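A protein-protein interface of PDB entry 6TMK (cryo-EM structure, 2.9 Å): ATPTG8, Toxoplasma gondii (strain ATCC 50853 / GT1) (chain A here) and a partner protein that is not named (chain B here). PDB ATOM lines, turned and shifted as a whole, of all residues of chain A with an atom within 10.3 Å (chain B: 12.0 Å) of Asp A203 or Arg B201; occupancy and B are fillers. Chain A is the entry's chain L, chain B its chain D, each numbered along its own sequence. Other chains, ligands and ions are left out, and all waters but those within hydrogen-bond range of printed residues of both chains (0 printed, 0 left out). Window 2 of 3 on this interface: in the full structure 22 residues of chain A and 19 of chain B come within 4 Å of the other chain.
Ala B197 touches Phe A195. CE2 of Phe A195 touches N of Asn B202, at 3.6 Å. Phe A195 touches Phe B203 (CE2 to N, 3.8 Å). Arg B201 touches Ala A199 (NH1 to O, 3.8 Å). Thr B198 touches Leu A202 (CG2 to CD1, 3.8 Å).
The side-chain carboxylate of Glu A42 is in salt-bridge range of the guanidinium group of Arg A198 (3.3 Å). OD1 of Asn B202 lies close to OD2 of Asp B204, at 3.1 Å. The backbone carbonyl oxygen (O) of Leu B194 sits at hydrogen-bond distance from the side-chain hydroxyl (OG1) of Thr B198. O of Ala B197 lies within hydrogen-bond range of N of Asn B202, at 3.3 Å.
Along chain A the printed residues that touch a printed residue of chain B span positions 195 to 203. Of the 18 printed residues of chain B, 5 touch a printed residue of chain A. Among the printed residues, 7 pairs touch across the chains.
Glu A42 touches none of the printed residues of chain B. Of the printed residues of chain B, Phe A195 touches Ala B197, Asn B202 and Phe B203. Of the printed residues of chain B, Arg A198 touches Thr B198. Of chain B, only Arg B201 comes within 4 Å of Ala A199. No residue of chain B comes within 4 Å of Val A200. Of the printed residues of chain B, Leu A202 touches Thr B198 (3.8 Å). Of chain B, only Arg B201 (3.3 Å) comes within 4 Å of Asp A203. No residue of chain B comes within 4 Å of Leu A204. No residue of chain B comes within 4 Å of Val A205. Of chain A, only Phe A195 (3.4 Å) comes within 4 Å of Ala B197. Of the printed residues of chain A, Thr B198 touches Arg A198 and Leu A202. No residue of chain A comes within 4 Å of Ala B200. Of the printed residues of chain A, Arg B201 touches Ala A199 and Asp A203. Asn B202 touches one residue of chain A. Printed residues of chain A within 4 Å of Phe B203: Phe A195 (3.8 Å). The nearest residue of chain B that does not touch Asp A203 is Thr B198 (7.7 Å).
The guanidinium group (NH1) of Arg A198 lies within hydrogen-bond range of the side-chain hydroxyl (OG1) of Thr B198 (2.6 Å). OD1 of Asp A203 lies within salt-bridge range of NH1 of Arg B201.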
ATOM      1  N   LEU A  34      12.468  27.729  16.215  1.00  0.00           N
ATOM      2  CA  LEU A  34      13.864  27.306  16.200  1.00  0.00           C
ATOM      3  C   LEU A  34      14.522  27.507  17.558  1.00  0.00           C
ATOM      4  O   LEU A  34      15.311  26.667  18.002  1.00  0.00           O
ATOM      5  CB  LEU A  34      14.636  28.055  15.120  1.00  0.00           C
ATOM      6  CG  LEU A  34      14.582  27.461  13.717  1.00  0.00           C
ATOM      7  CD1 LEU A  34      13.238  27.641  13.056  1.00  0.00           C
ATOM      8  CD2 LEU A  34      15.671  28.100  12.898  1.00  0.00           C
ATOM      9  N   LEU A  38      16.251  24.689  19.871  1.00  0.00           N
ATOM     10  CA  LEU A  38      17.620  24.831  20.345  1.00  0.00           C
ATOM     11  C   LEU A  38      17.710  24.618  21.845  1.00  0.00           C
ATOM     12  O   LEU A  38      18.634  23.955  22.330  1.00  0.00           O
ATOM     13  CB  LEU A  38      18.159  26.209  19.988  1.00  0.00           C
ATOM     14  CG  LEU A  38      18.564  26.458  18.544  1.00  0.00           C
ATOM     15  CD1 LEU A  38      19.051  27.875  18.424  1.00  0.00           C
ATOM     16  CD2 LEU A  38      19.631  25.492  18.110  1.00  0.00           C
ATOM     17  N   GLU A  42      19.848  21.808  23.857  1.00  0.00           N
ATOM     18  CA  GLU A  42      20.840  22.141  24.871  1.00  0.00           C
ATOM     19  C   GLU A  42      20.538  21.434  26.183  1.00  0.00           C
ATOM     20  O   GLU A  42      21.455  21.014  26.895  1.00  0.00           O
ATOM     21  CB  GLU A  42      20.897  23.649  25.081  1.00  0.00           C
ATOM     22  CG  GLU A  42      21.494  24.402  23.921  1.00  0.00           C
ATOM     23  CD  GLU A  42      21.362  25.901  24.068  1.00  0.00           C
ATOM     24  OE1 GLU A  42      20.939  26.358  25.150  1.00  0.00           O
ATOM     25  OE2 GLU A  42      21.681  26.624  23.101  1.00  0.00           O
ATOM     26  N   LYS A 192      26.578  13.642  19.901  1.00  0.00           N
ATOM     27  CA  LYS A 192      27.262  14.243  18.761  1.00  0.00           C
ATOM     28  C   LYS A 192      26.266  14.672  17.691  1.00  0.00           C
ATOM     29  O   LYS A 192      26.369  15.774  17.129  1.00  0.00           O
ATOM     30  CB  LYS A 192      28.274  13.256  18.192  1.00  0.00           C
ATOM     31  CG  LYS A 192      29.463  13.891  17.529  1.00  0.00           C
ATOM     32  CD  LYS A 192      30.483  12.849  17.159  1.00  0.00           C
ATOM     33  CE  LYS A 192      31.557  13.415  16.256  1.00  0.00           C
ATOM     34  NZ  LYS A 192      32.488  12.355  15.779  1.00  0.00           N
ATOM     35  N   LEU A 194      23.116  15.440  18.097  1.00  0.00           N
ATOM     36  CA  LEU A 194      22.423  16.620  18.605  1.00  0.00           C
ATOM     37  C   LEU A 194      23.275  17.870  18.451  1.00  0.00           C
ATOM     38  O   LEU A 194      22.761  18.951  18.141  1.00  0.00           O
ATOM     39  CB  LEU A 194      22.053  16.421  20.070  1.00  0.00           C
ATOM     40  CG  LEU A 194      20.990  15.386  20.417  1.00  0.00           C
ATOM     41  CD1 LEU A 194      20.701  15.458  21.888  1.00  0.00           C
ATOM     42  CD2 LEU A 194      19.725  15.614  19.633  1.00  0.00           C
ATOM     43  N   PHE A 195      24.582  17.745  18.671  1.00  0.00           N
ATOM     44  CA  PHE A 195      25.465  18.895  18.529  1.00  0.00           C
ATOM     45  C   PHE A 195      25.480  19.402  17.094  1.00  0.00           C
ATOM     46  O   PHE A 195      25.434  20.614  16.851  1.00  0.00           O
ATOM     47  CB  PHE A 195      26.870  18.520  18.983  1.00  0.00           C
ATOM     48  CG  PHE A 195      27.778  19.690  19.170  1.00  0.00           C
ATOM     49  CD1 PHE A 195      27.695  20.467  20.304  1.00  0.00           C
ATOM     50  CD2 PHE A 195      28.716  20.013  18.214  1.00  0.00           C
ATOM     51  CE1 PHE A 195      28.528  21.541  20.481  1.00  0.00           C
ATOM     52  CE2 PHE A 195      29.551  21.087  18.388  1.00  0.00           C
ATOM     53  CZ  PHE A 195      29.454  21.851  19.523  1.00  0.00           C
ATOM     54  N   GLU A 196      25.547  18.490  16.125  1.00  0.00           N
ATOM     55  CA  GLU A 196      25.542  18.920  14.728  1.00  0.00           C
ATOM     56  C   GLU A 196      24.203  19.544  14.340  1.00  0.00           C
ATOM     57  O   GLU A 196      24.156  20.526  13.583  1.00  0.00           O
ATOM     58  CB  GLU A 196      25.869  17.741  13.816  1.00  0.00           C
ATOM     59  CG  GLU A 196      27.145  17.009  14.183  1.00  0.00           C
ATOM     60  CD  GLU A 196      28.299  17.942  14.484  1.00  0.00           C
ATOM     61  OE1 GLU A 196      28.422  18.980  13.800  1.00  0.00           O
ATOM     62  OE2 GLU A 196      29.086  17.638  15.405  1.00  0.00           O
ATOM     63  N   ARG A 197      23.103  18.984  14.845  1.00  0.00           N
ATOM     64  CA  ARG A 197      21.793  19.587  14.613  1.00  0.00           C
ATOM     65  C   ARG A 197      21.744  21.007  15.162  1.00  0.00           C
ATOM     66  O   ARG A 197      21.234  21.926  14.504  1.00  0.00           O
ATOM     67  CB  ARG A 197      20.711  18.714  15.249  1.00  0.00           C
ATOM     68  CG  ARG A 197      19.308  19.275  15.189  1.00  0.00           C
ATOM     69  CD  ARG A 197      18.877  19.595  13.778  1.00  0.00           C
ATOM     70  NE  ARG A 197      17.463  19.943  13.711  1.00  0.00           N
ATOM     71  CZ  ARG A 197      16.882  20.518  12.663  1.00  0.00           C
ATOM     72  NH1 ARG A 197      17.595  20.816  11.588  1.00  0.00           N
ATOM     73  NH2 ARG A 197      15.588  20.799  12.691  1.00  0.00           N
ATOM     74  N   ARG A 198      22.286  21.207  16.361  1.00  0.00           N
ATOM     75  CA  ARG A 198      22.370  22.545  16.928  1.00  0.00           C
ATOM     76  C   ARG A 198      23.210  23.461  16.054  1.00  0.00           C
ATOM     77  O   ARG A 198      22.900  24.645  15.908  1.00  0.00           O
ATOM     78  CB  ARG A 198      22.951  22.477  18.332  1.00  0.00           C
ATOM     79  CG  ARG A 198      23.053  23.807  19.014  1.00  0.00           C
ATOM     80  CD  ARG A 198      23.390  23.641  20.461  1.00  0.00           C
ATOM     81  NE  ARG A 198      23.676  24.909  21.116  1.00  0.00           N
ATOM     82  CZ  ARG A 198      24.862  25.501  21.107  1.00  0.00           C
ATOM     83  NH1 ARG A 198      25.885  24.953  20.472  1.00  0.00           N
ATOM     84  NH2 ARG A 198      25.027  26.650  21.731  1.00  0.00           N
ATOM     85  N   ALA A 199      24.291  22.936  15.484  1.00  0.00           N
ATOM     86  CA  ALA A 199      25.155  23.761  14.651  1.00  0.00           C
ATOM     87  C   ALA A 199      24.407  24.269  13.425  1.00  0.00           C
ATOM     88  O   ALA A 199      24.471  25.459  13.085  1.00  0.00           O
ATOM     89  CB  ALA A 199      26.388  22.967  14.235  1.00  0.00           C
ATOM     90  N   VAL A 200      23.678  23.382  12.750  1.00  0.00           N
ATOM     91  CA  VAL A 200      22.951  23.819  11.562  1.00  0.00           C
ATOM     92  C   VAL A 200      21.828  24.775  11.948  1.00  0.00           C
ATOM     93  O   VAL A 200      21.545  25.748  11.234  1.00  0.00           O
ATOM     94  CB  VAL A 200      22.424  22.613  10.763  1.00  0.00           C
ATOM     95  CG1 VAL A 200      23.565  21.695  10.392  1.00  0.00           C
ATOM     96  CG2 VAL A 200      21.371  21.865  11.527  1.00  0.00           C
ATOM     97  N   LEU A 201      21.184  24.540  13.092  1.00  0.00           N
ATOM     98  CA  LEU A 201      20.127  25.451  13.513  1.00  0.00           C
ATOM     99  C   LEU A 201      20.675  26.811  13.917  1.00  0.00           C
ATOM    100  O   LEU A 201      19.975  27.819  13.784  1.00  0.00           O
ATOM    101  CB  LEU A 201      19.334  24.858  14.669  1.00  0.00           C
ATOM    102  CG  LEU A 201      18.392  23.699  14.381  1.00  0.00           C
ATOM    103  CD1 LEU A 201      17.536  23.476  15.593  1.00  0.00           C
ATOM    104  CD2 LEU A 201      17.535  23.976  13.170  1.00  0.00           C
ATOM    105  N   LEU A 202      21.908  26.867  14.408  1.00  0.00           N
ATOM    106  CA  LEU A 202      22.523  28.154  14.701  1.00  0.00           C
ATOM    107  C   LEU A 202      22.991  28.860  13.441  1.00  0.00           C
ATOM    108  O   LEU A 202      23.069  30.092  13.419  1.00  0.00           O
ATOM    109  CB  LEU A 202      23.709  27.972  15.639  1.00  0.00           C
ATOM    110  CG  LEU A 202      23.429  27.581  17.084  1.00  0.00           C
ATOM    111  CD1 LEU A 202      24.735  27.364  17.797  1.00  0.00           C
ATOM    112  CD2 LEU A 202      22.609  28.626  17.783  1.00  0.00           C
ATOM    113  N   ASP A 203      23.310  28.105  12.393  1.00  0.00           N
ATOM    114  CA  ASP A 203      23.554  28.739  11.103  1.00  0.00           C
ATOM    115  C   ASP A 203      22.268  29.287  10.499  1.00  0.00           C
ATOM    116  O   ASP A 203      22.302  30.292   9.781  1.00  0.00           O
ATOM    117  CB  ASP A 203      24.215  27.755  10.143  1.00  0.00           C
ATOM    118  CG  ASP A 203      25.639  27.425  10.540  1.00  0.00           C
ATOM    119  OD1 ASP A 203      25.948  27.479  11.748  1.00  0.00           O
ATOM    120  OD2 ASP A 203      26.450  27.115   9.643  1.00  0.00           O
ATOM    121  N   LEU A 204      21.133  28.648  10.774  1.00  0.00           N
ATOM    122  CA  LEU A 204      19.858  29.119  10.248  1.00  0.00           C
ATOM    123  C   LEU A 204      19.179  30.155  11.131  1.00  0.00           C
ATOM    124  O   LEU A 204      18.244  30.819  10.671  1.00  0.00           O
ATOM    125  CB  LEU A 204      18.891  27.949  10.057  1.00  0.00           C
ATOM    126  CG  LEU A 204      19.247  26.902   9.009  1.00  0.00           C
ATOM    127  CD1 LEU A 204      18.206  25.804   9.019  1.00  0.00           C
ATOM    128  CD2 LEU A 204      19.342  27.537   7.641  1.00  0.00           C
ATOM    129  N   VAL A 205      19.610  30.305  12.380  1.00  0.00           N
ATOM    130  CA  VAL A 205      18.893  31.176  13.300  1.00  0.00           C
ATOM    131  C   VAL A 205      19.009  32.627  12.848  1.00  0.00           C
ATOM    132  O   VAL A 205      19.944  33.025  12.146  1.00  0.00           O
ATOM    133  CB  VAL A 205      19.407  31.001  14.738  1.00  0.00           C
ATOM    134  CG1 VAL A 205      20.741  31.680  14.913  1.00  0.00           C
ATOM    135  CG2 VAL A 205      18.409  31.544  15.723  1.00  0.00           C
ATOM    136  N   GLU A 206      18.035  33.428  13.267  1.00  0.00           N
ATOM    137  CA  GLU A 206      17.802  34.734  12.676  1.00  0.00           C
ATOM    138  C   GLU A 206      17.329  35.697  13.750  1.00  0.00           C
ATOM    139  O   GLU A 206      16.479  35.355  14.576  1.00  0.00           O
ATOM    140  CB  GLU A 206      16.774  34.665  11.544  1.00  0.00           C
ATOM    141  CG  GLU A 206      16.684  35.933  10.729  1.00  0.00           C
ATOM    142  CD  GLU A 206      16.135  35.696   9.339  1.00  0.00           C
ATOM    143  OE1 GLU A 206      15.620  34.587   9.083  1.00  0.00           O
ATOM    144  OE2 GLU A 206      16.221  36.617   8.500  1.00  0.00           O
ATOM    145  N   GLY A 207      17.886  36.899  13.725  1.00  0.00           N
ATOM    146  CA  GLY A 207      17.660  37.911  14.730  1.00  0.00           C
ATOM    147  C   GLY A 207      18.957  38.552  15.164  1.00  0.00           C
ATOM    148  O   GLY A 207      20.038  38.245  14.665  1.00  0.00           O
ATOM    149  N   GLU B 192      30.639  27.264  30.426  1.00  0.00           N
ATOM    150  CA  GLU B 192      31.888  27.588  29.747  1.00  0.00           C
ATOM    151  C   GLU B 192      32.149  26.643  28.579  1.00  0.00           C
ATOM    152  O   GLU B 192      32.518  27.078  27.477  1.00  0.00           O
ATOM    153  CB  GLU B 192      33.038  27.536  30.745  1.00  0.00           C
ATOM    154  CG  GLU B 192      34.317  28.152  30.259  1.00  0.00           C
ATOM    155  CD  GLU B 192      35.403  28.098  31.303  1.00  0.00           C
ATOM    156  OE1 GLU B 192      35.213  27.385  32.311  1.00  0.00           O
ATOM    157  OE2 GLU B 192      36.441  28.767  31.122  1.00  0.00           O
ATOM    158  N   ALA B 193      31.977  25.341  28.806  1.00  0.00           N
ATOM    159  CA  ALA B 193      32.234  24.358  27.765  1.00  0.00           C
ATOM    160  C   ALA B 193      31.321  24.565  26.571  1.00  0.00           C
ATOM    161  O   ALA B 193      31.765  24.487  25.422  1.00  0.00           O
ATOM    162  CB  ALA B 193      32.055  22.952  28.329  1.00  0.00           C
ATOM    163  N   LEU B 194      30.039  24.814  26.820  1.00  0.00           N
ATOM    164  CA  LEU B 194      29.107  25.010  25.722  1.00  0.00           C
ATOM    165  C   LEU B 194      29.435  26.270  24.942  1.00  0.00           C
ATOM    166  O   LEU B 194      29.354  26.280  23.711  1.00  0.00           O
ATOM    167  CB  LEU B 194      27.680  25.060  26.249  1.00  0.00           C
ATOM    168  CG  LEU B 194      26.603  25.090  25.175  1.00  0.00           C
ATOM    169  CD1 LEU B 194      26.578  23.796  24.396  1.00  0.00           C
ATOM    170  CD2 LEU B 194      25.269  25.357  25.795  1.00  0.00           C
ATOM    171  N   ARG B 195      29.837  27.338  25.629  1.00  0.00           N
ATOM    172  CA  ARG B 195      30.208  28.559  24.923  1.00  0.00           C
ATOM    173  C   ARG B 195      31.406  28.323  24.012  1.00  0.00           C
ATOM    174  O   ARG B 195      31.395  28.700  22.830  1.00  0.00           O
ATOM    175  CB  ARG B 195      30.500  29.669  25.927  1.00  0.00           C
ATOM    176  CG  ARG B 195      29.261  30.352  26.427  1.00  0.00           C
ATOM    177  CD  ARG B 195      29.574  31.624  27.169  1.00  0.00           C
ATOM    178  NE  ARG B 195      29.680  31.425  28.610  1.00  0.00           N
ATOM    179  CZ  ARG B 195      30.823  31.325  29.279  1.00  0.00           C
ATOM    180  NH1 ARG B 195      31.985  31.398  28.654  1.00  0.00           N
ATOM    181  NH2 ARG B 195      30.801  31.147  30.584  1.00  0.00           N
ATOM    182  N   GLU B 196      32.456  27.704  24.551  1.00  0.00           N
ATOM    183  CA  GLU B 196      33.659  27.476  23.763  1.00  0.00           C
ATOM    184  C   GLU B 196      33.399  26.520  22.606  1.00  0.00           C
ATOM    185  O   GLU B 196      33.862  26.754  21.483  1.00  0.00           O
ATOM    186  CB  GLU B 196      34.764  26.945  24.665  1.00  0.00           C
ATOM    187  CG  GLU B 196      35.264  27.963  25.661  1.00  0.00           C
ATOM    188  CD  GLU B 196      36.320  28.891  25.088  1.00  0.00           C
ATOM    189  OE1 GLU B 196      36.981  28.511  24.099  1.00  0.00           O
ATOM    190  OE2 GLU B 196      36.492  30.002  25.633  1.00  0.00           O
ATOM    191  N   ALA B 197      32.639  25.454  22.850  1.00  0.00           N
ATOM    192  CA  ALA B 197      32.327  24.511  21.790  1.00  0.00           C
ATOM    193  C   ALA B 197      31.376  25.092  20.761  1.00  0.00           C
ATOM    194  O   ALA B 197      31.364  24.625  19.624  1.00  0.00           O
ATOM    195  CB  ALA B 197      31.721  23.244  22.383  1.00  0.00           C
ATOM    196  N   THR B 198      30.587  26.098  21.127  1.00  0.00           N
ATOM    197  CA  THR B 198      29.722  26.742  20.152  1.00  0.00           C
ATOM    198  C   THR B 198      30.505  27.697  19.268  1.00  0.00           C
ATOM    199  O   THR B 198      30.263  27.765  18.059  1.00  0.00           O
ATOM    200  CB  THR B 198      28.591  27.484  20.858  1.00  0.00           C
ATOM    201  OG1 THR B 198      27.710  26.542  21.479  1.00  0.00           O
ATOM    202  CG2 THR B 198      27.815  28.327  19.872  1.00  0.00           C
ATOM    203  N   LEU B 199      31.449  28.445  19.844  1.00  0.00           N
ATOM    204  CA  LEU B 199      32.229  29.341  19.000  1.00  0.00           C
ATOM    205  C   LEU B 199      33.219  28.571  18.136  1.00  0.00           C
ATOM    206  O   LEU B 199      33.544  29.015  17.030  1.00  0.00           O
ATOM    207  CB  LEU B 199      32.963  30.392  19.835  1.00  0.00           C
ATOM    208  CG  LEU B 199      34.068  29.949  20.787  1.00  0.00           C
ATOM    209  CD1 LEU B 199      35.391  29.830  20.061  1.00  0.00           C
ATOM    210  CD2 LEU B 199      34.200  30.941  21.910  1.00  0.00           C
ATOM    211  N   ALA B 200      33.704  27.425  18.611  1.00  0.00           N
ATOM    212  CA  ALA B 200      34.598  26.595  17.817  1.00  0.00           C
ATOM    213  C   ALA B 200      33.864  25.647  16.880  1.00  0.00           C
ATOM    214  O   ALA B 200      34.451  25.202  15.888  1.00  0.00           O
ATOM    215  CB  ALA B 200      35.509  25.777  18.731  1.00  0.00           C
ATOM    216  N   ARG B 201      32.604  25.335  17.166  1.00  0.00           N
ATOM    217  CA  ARG B 201      31.841  24.329  16.438  1.00  0.00           C
ATOM    218  C   ARG B 201      32.607  23.009  16.380  1.00  0.00           C
ATOM    219  O   ARG B 201      32.998  22.519  15.320  1.00  0.00           O
ATOM    220  CB  ARG B 201      31.476  24.844  15.051  1.00  0.00           C
ATOM    221  CG  ARG B 201      30.259  25.736  15.098  1.00  0.00           C
ATOM    222  CD  ARG B 201      30.171  26.679  13.927  1.00  0.00           C
ATOM    223  NE  ARG B 201      29.589  27.951  14.339  1.00  0.00           N
ATOM    224  CZ  ARG B 201      28.316  28.107  14.684  1.00  0.00           C
ATOM    225  NH1 ARG B 201      27.489  27.075  14.661  1.00  0.00           N
ATOM    226  NH2 ARG B 201      27.867  29.297  15.049  1.00  0.00           N
ATOM    227  N   ASN B 202      32.807  22.436  17.565  1.00  0.00           N
ATOM    228  CA  ASN B 202      33.545  21.189  17.703  1.00  0.00           C
ATOM    229  C   ASN B 202      33.108  20.487  18.981  1.00  0.00           C
ATOM    230  O   ASN B 202      33.045  21.107  20.044  1.00  0.00           O
ATOM    231  CB  ASN B 202      35.049  21.453  17.721  1.00  0.00           C
ATOM    232  CG  ASN B 202      35.861  20.209  17.461  1.00  0.00           C
ATOM    233  OD1 ASN B 202      35.338  19.193  17.005  1.00  0.00           O
ATOM    234  ND2 ASN B 202      37.150  20.282  17.745  1.00  0.00           N
ATOM    235  N   PHE B 203      32.811  19.193  18.861  1.00  0.00           N
ATOM    236  CA  PHE B 203      32.368  18.371  19.983  1.00  0.00           C
ATOM    237  C   PHE B 203      33.534  17.905  20.848  1.00  0.00           C
ATOM    238  O   PHE B 203      33.361  17.650  22.050  1.00  0.00           O
ATOM    239  CB  PHE B 203      31.589  17.178  19.432  1.00  0.00           C
ATOM    240  CG  PHE B 203      30.955  16.323  20.475  1.00  0.00           C
ATOM    241  CD1 PHE B 203      29.811  16.731  21.120  1.00  0.00           C
ATOM    242  CD2 PHE B 203      31.489  15.092  20.792  1.00  0.00           C
ATOM    243  CE1 PHE B 203      29.223  15.941  22.069  1.00  0.00           C
ATOM    244  CE2 PHE B 203      30.904  14.300  21.743  1.00  0.00           C
ATOM    245  CZ  PHE B 203      29.768  14.725  22.382  1.00  0.00           C
ATOM    246  N   ASP B 204      34.723  17.793  20.260  1.00  0.00           N
ATOM    247  CA  ASP B 204      35.899  17.410  21.026  1.00  0.00           C
ATOM    248  C   ASP B 204      36.191  18.404  22.139  1.00  0.00           C
ATOM    249  O   ASP B 204      36.789  18.039  23.152  1.00  0.00           O
ATOM    250  CB  ASP B 204      37.099  17.277  20.096  1.00  0.00           C
ATOM    251  CG  ASP B 204      36.923  16.165  19.080  1.00  0.00           C
ATOM    252  OD1 ASP B 204      37.198  14.997  19.421  1.00  0.00           O
ATOM    253  OD2 ASP B 204      36.507  16.460  17.941  1.00  0.00           O
ATOM    254  N   VAL B 205      35.785  19.658  21.971  1.00  0.00           N
ATOM    255  CA  VAL B 205      35.991  20.657  23.015  1.00  0.00           C
ATOM    256  C   VAL B 205      35.131  20.339  24.234  1.00  0.00           C
ATOM    257  O   VAL B 205      35.610  20.331  25.377  1.00  0.00           O
ATOM    258  CB  VAL B 205      35.701  22.060  22.460  1.00  0.00           C
ATOM    259  CG1 VAL B 205      35.837  23.095  23.535  1.00  0.00           C
ATOM    260  CG2 VAL B 205      36.638  22.367  21.319  1.00  0.00           C
ATOM    261  N   LEU B 206      33.836  20.114  24.009  1.00  0.00           N
ATOM    262  CA  LEU B 206      32.971  19.619  25.071  1.00  0.00           C
ATOM    263  C   LEU B 206      33.574  18.401  25.748  1.00  0.00           C
ATOM    264  O   LEU B 206      33.572  18.295  26.979  1.00  0.00           O
ATOM    265  CB  LEU B 206      31.606  19.253  24.495  1.00  0.00           C
ATOM    266  CG  LEU B 206      30.484  20.274  24.411  1.00  0.00           C
ATOM    267  CD1 LEU B 206      29.220  19.564  24.022  1.00  0.00           C
ATOM    268  CD2 LEU B 206      30.282  20.995  25.702  1.00  0.00           C
ATOM    269  N   VAL B 207      34.089  17.464  24.953  1.00  0.00           N
ATOM    270  CA  VAL B 207      34.697  16.266  25.525  1.00  0.00           C
ATOM    271  C   VAL B 207      35.903  16.622  26.389  1.00  0.00           C
ATOM    272  O   VAL B 207      36.124  16.021  27.445  1.00  0.00           O
ATOM    273  CB  VAL B 207      35.071  15.278  24.410  1.00  0.00           C
ATOM    274  CG1 VAL B 207      35.890  14.146  24.971  1.00  0.00           C
ATOM    275  CG2 VAL B 207      33.826  14.746  23.762  1.00  0.00           C
ATOM    276  N   SER B 208      36.703  17.593  25.953  1.00  0.00           N
ATOM    277  CA  SER B 208      37.892  17.973  26.701  1.00  0.00           C
ATOM    278  C   SER B 208      37.564  18.709  27.987  1.00  0.00           C
ATOM    279  O   SER B 208      38.395  18.733  28.899  1.00  0.00           O
ATOM    280  CB  SER B 208      38.793  18.840  25.831  1.00  0.00           C
ATOM    281  OG  SER B 208      38.219  20.115  25.635  1.00  0.00           O
ATOM    282  N   TYR B 209      36.389  19.318  28.079  1.00  0.00           N
ATOM    283  CA  TYR B 209      35.983  19.913  29.349  1.00  0.00           C
ATOM    284  C   TYR B 209      35.518  18.889  30.375  1.00  0.00           C
ATOM    285  O   TYR B 209      35.137  19.284  31.481  1.00  0.00           O
ATOM    286  CB  TYR B 209      34.905  20.974  29.133  1.00  0.00           C
ATOM    287  CG  TYR B 209      35.429  22.267  28.563  1.00  0.00           C
ATOM    288  CD1 TYR B 209      36.061  23.180  29.385  1.00  0.00           C
ATOM    289  CD2 TYR B 209      35.324  22.566  27.219  1.00  0.00           C
ATOM    290  CE1 TYR B 209      36.550  24.359  28.899  1.00  0.00           C
ATOM    291  CE2 TYR B 209      35.817  23.750  26.721  1.00  0.00           C
ATOM    292  CZ  TYR B 209      36.439  24.638  27.567  1.00  0.00           C
ATOM    293  OH  TYR B 209      36.939  25.823  27.086  1.00  0.00           O
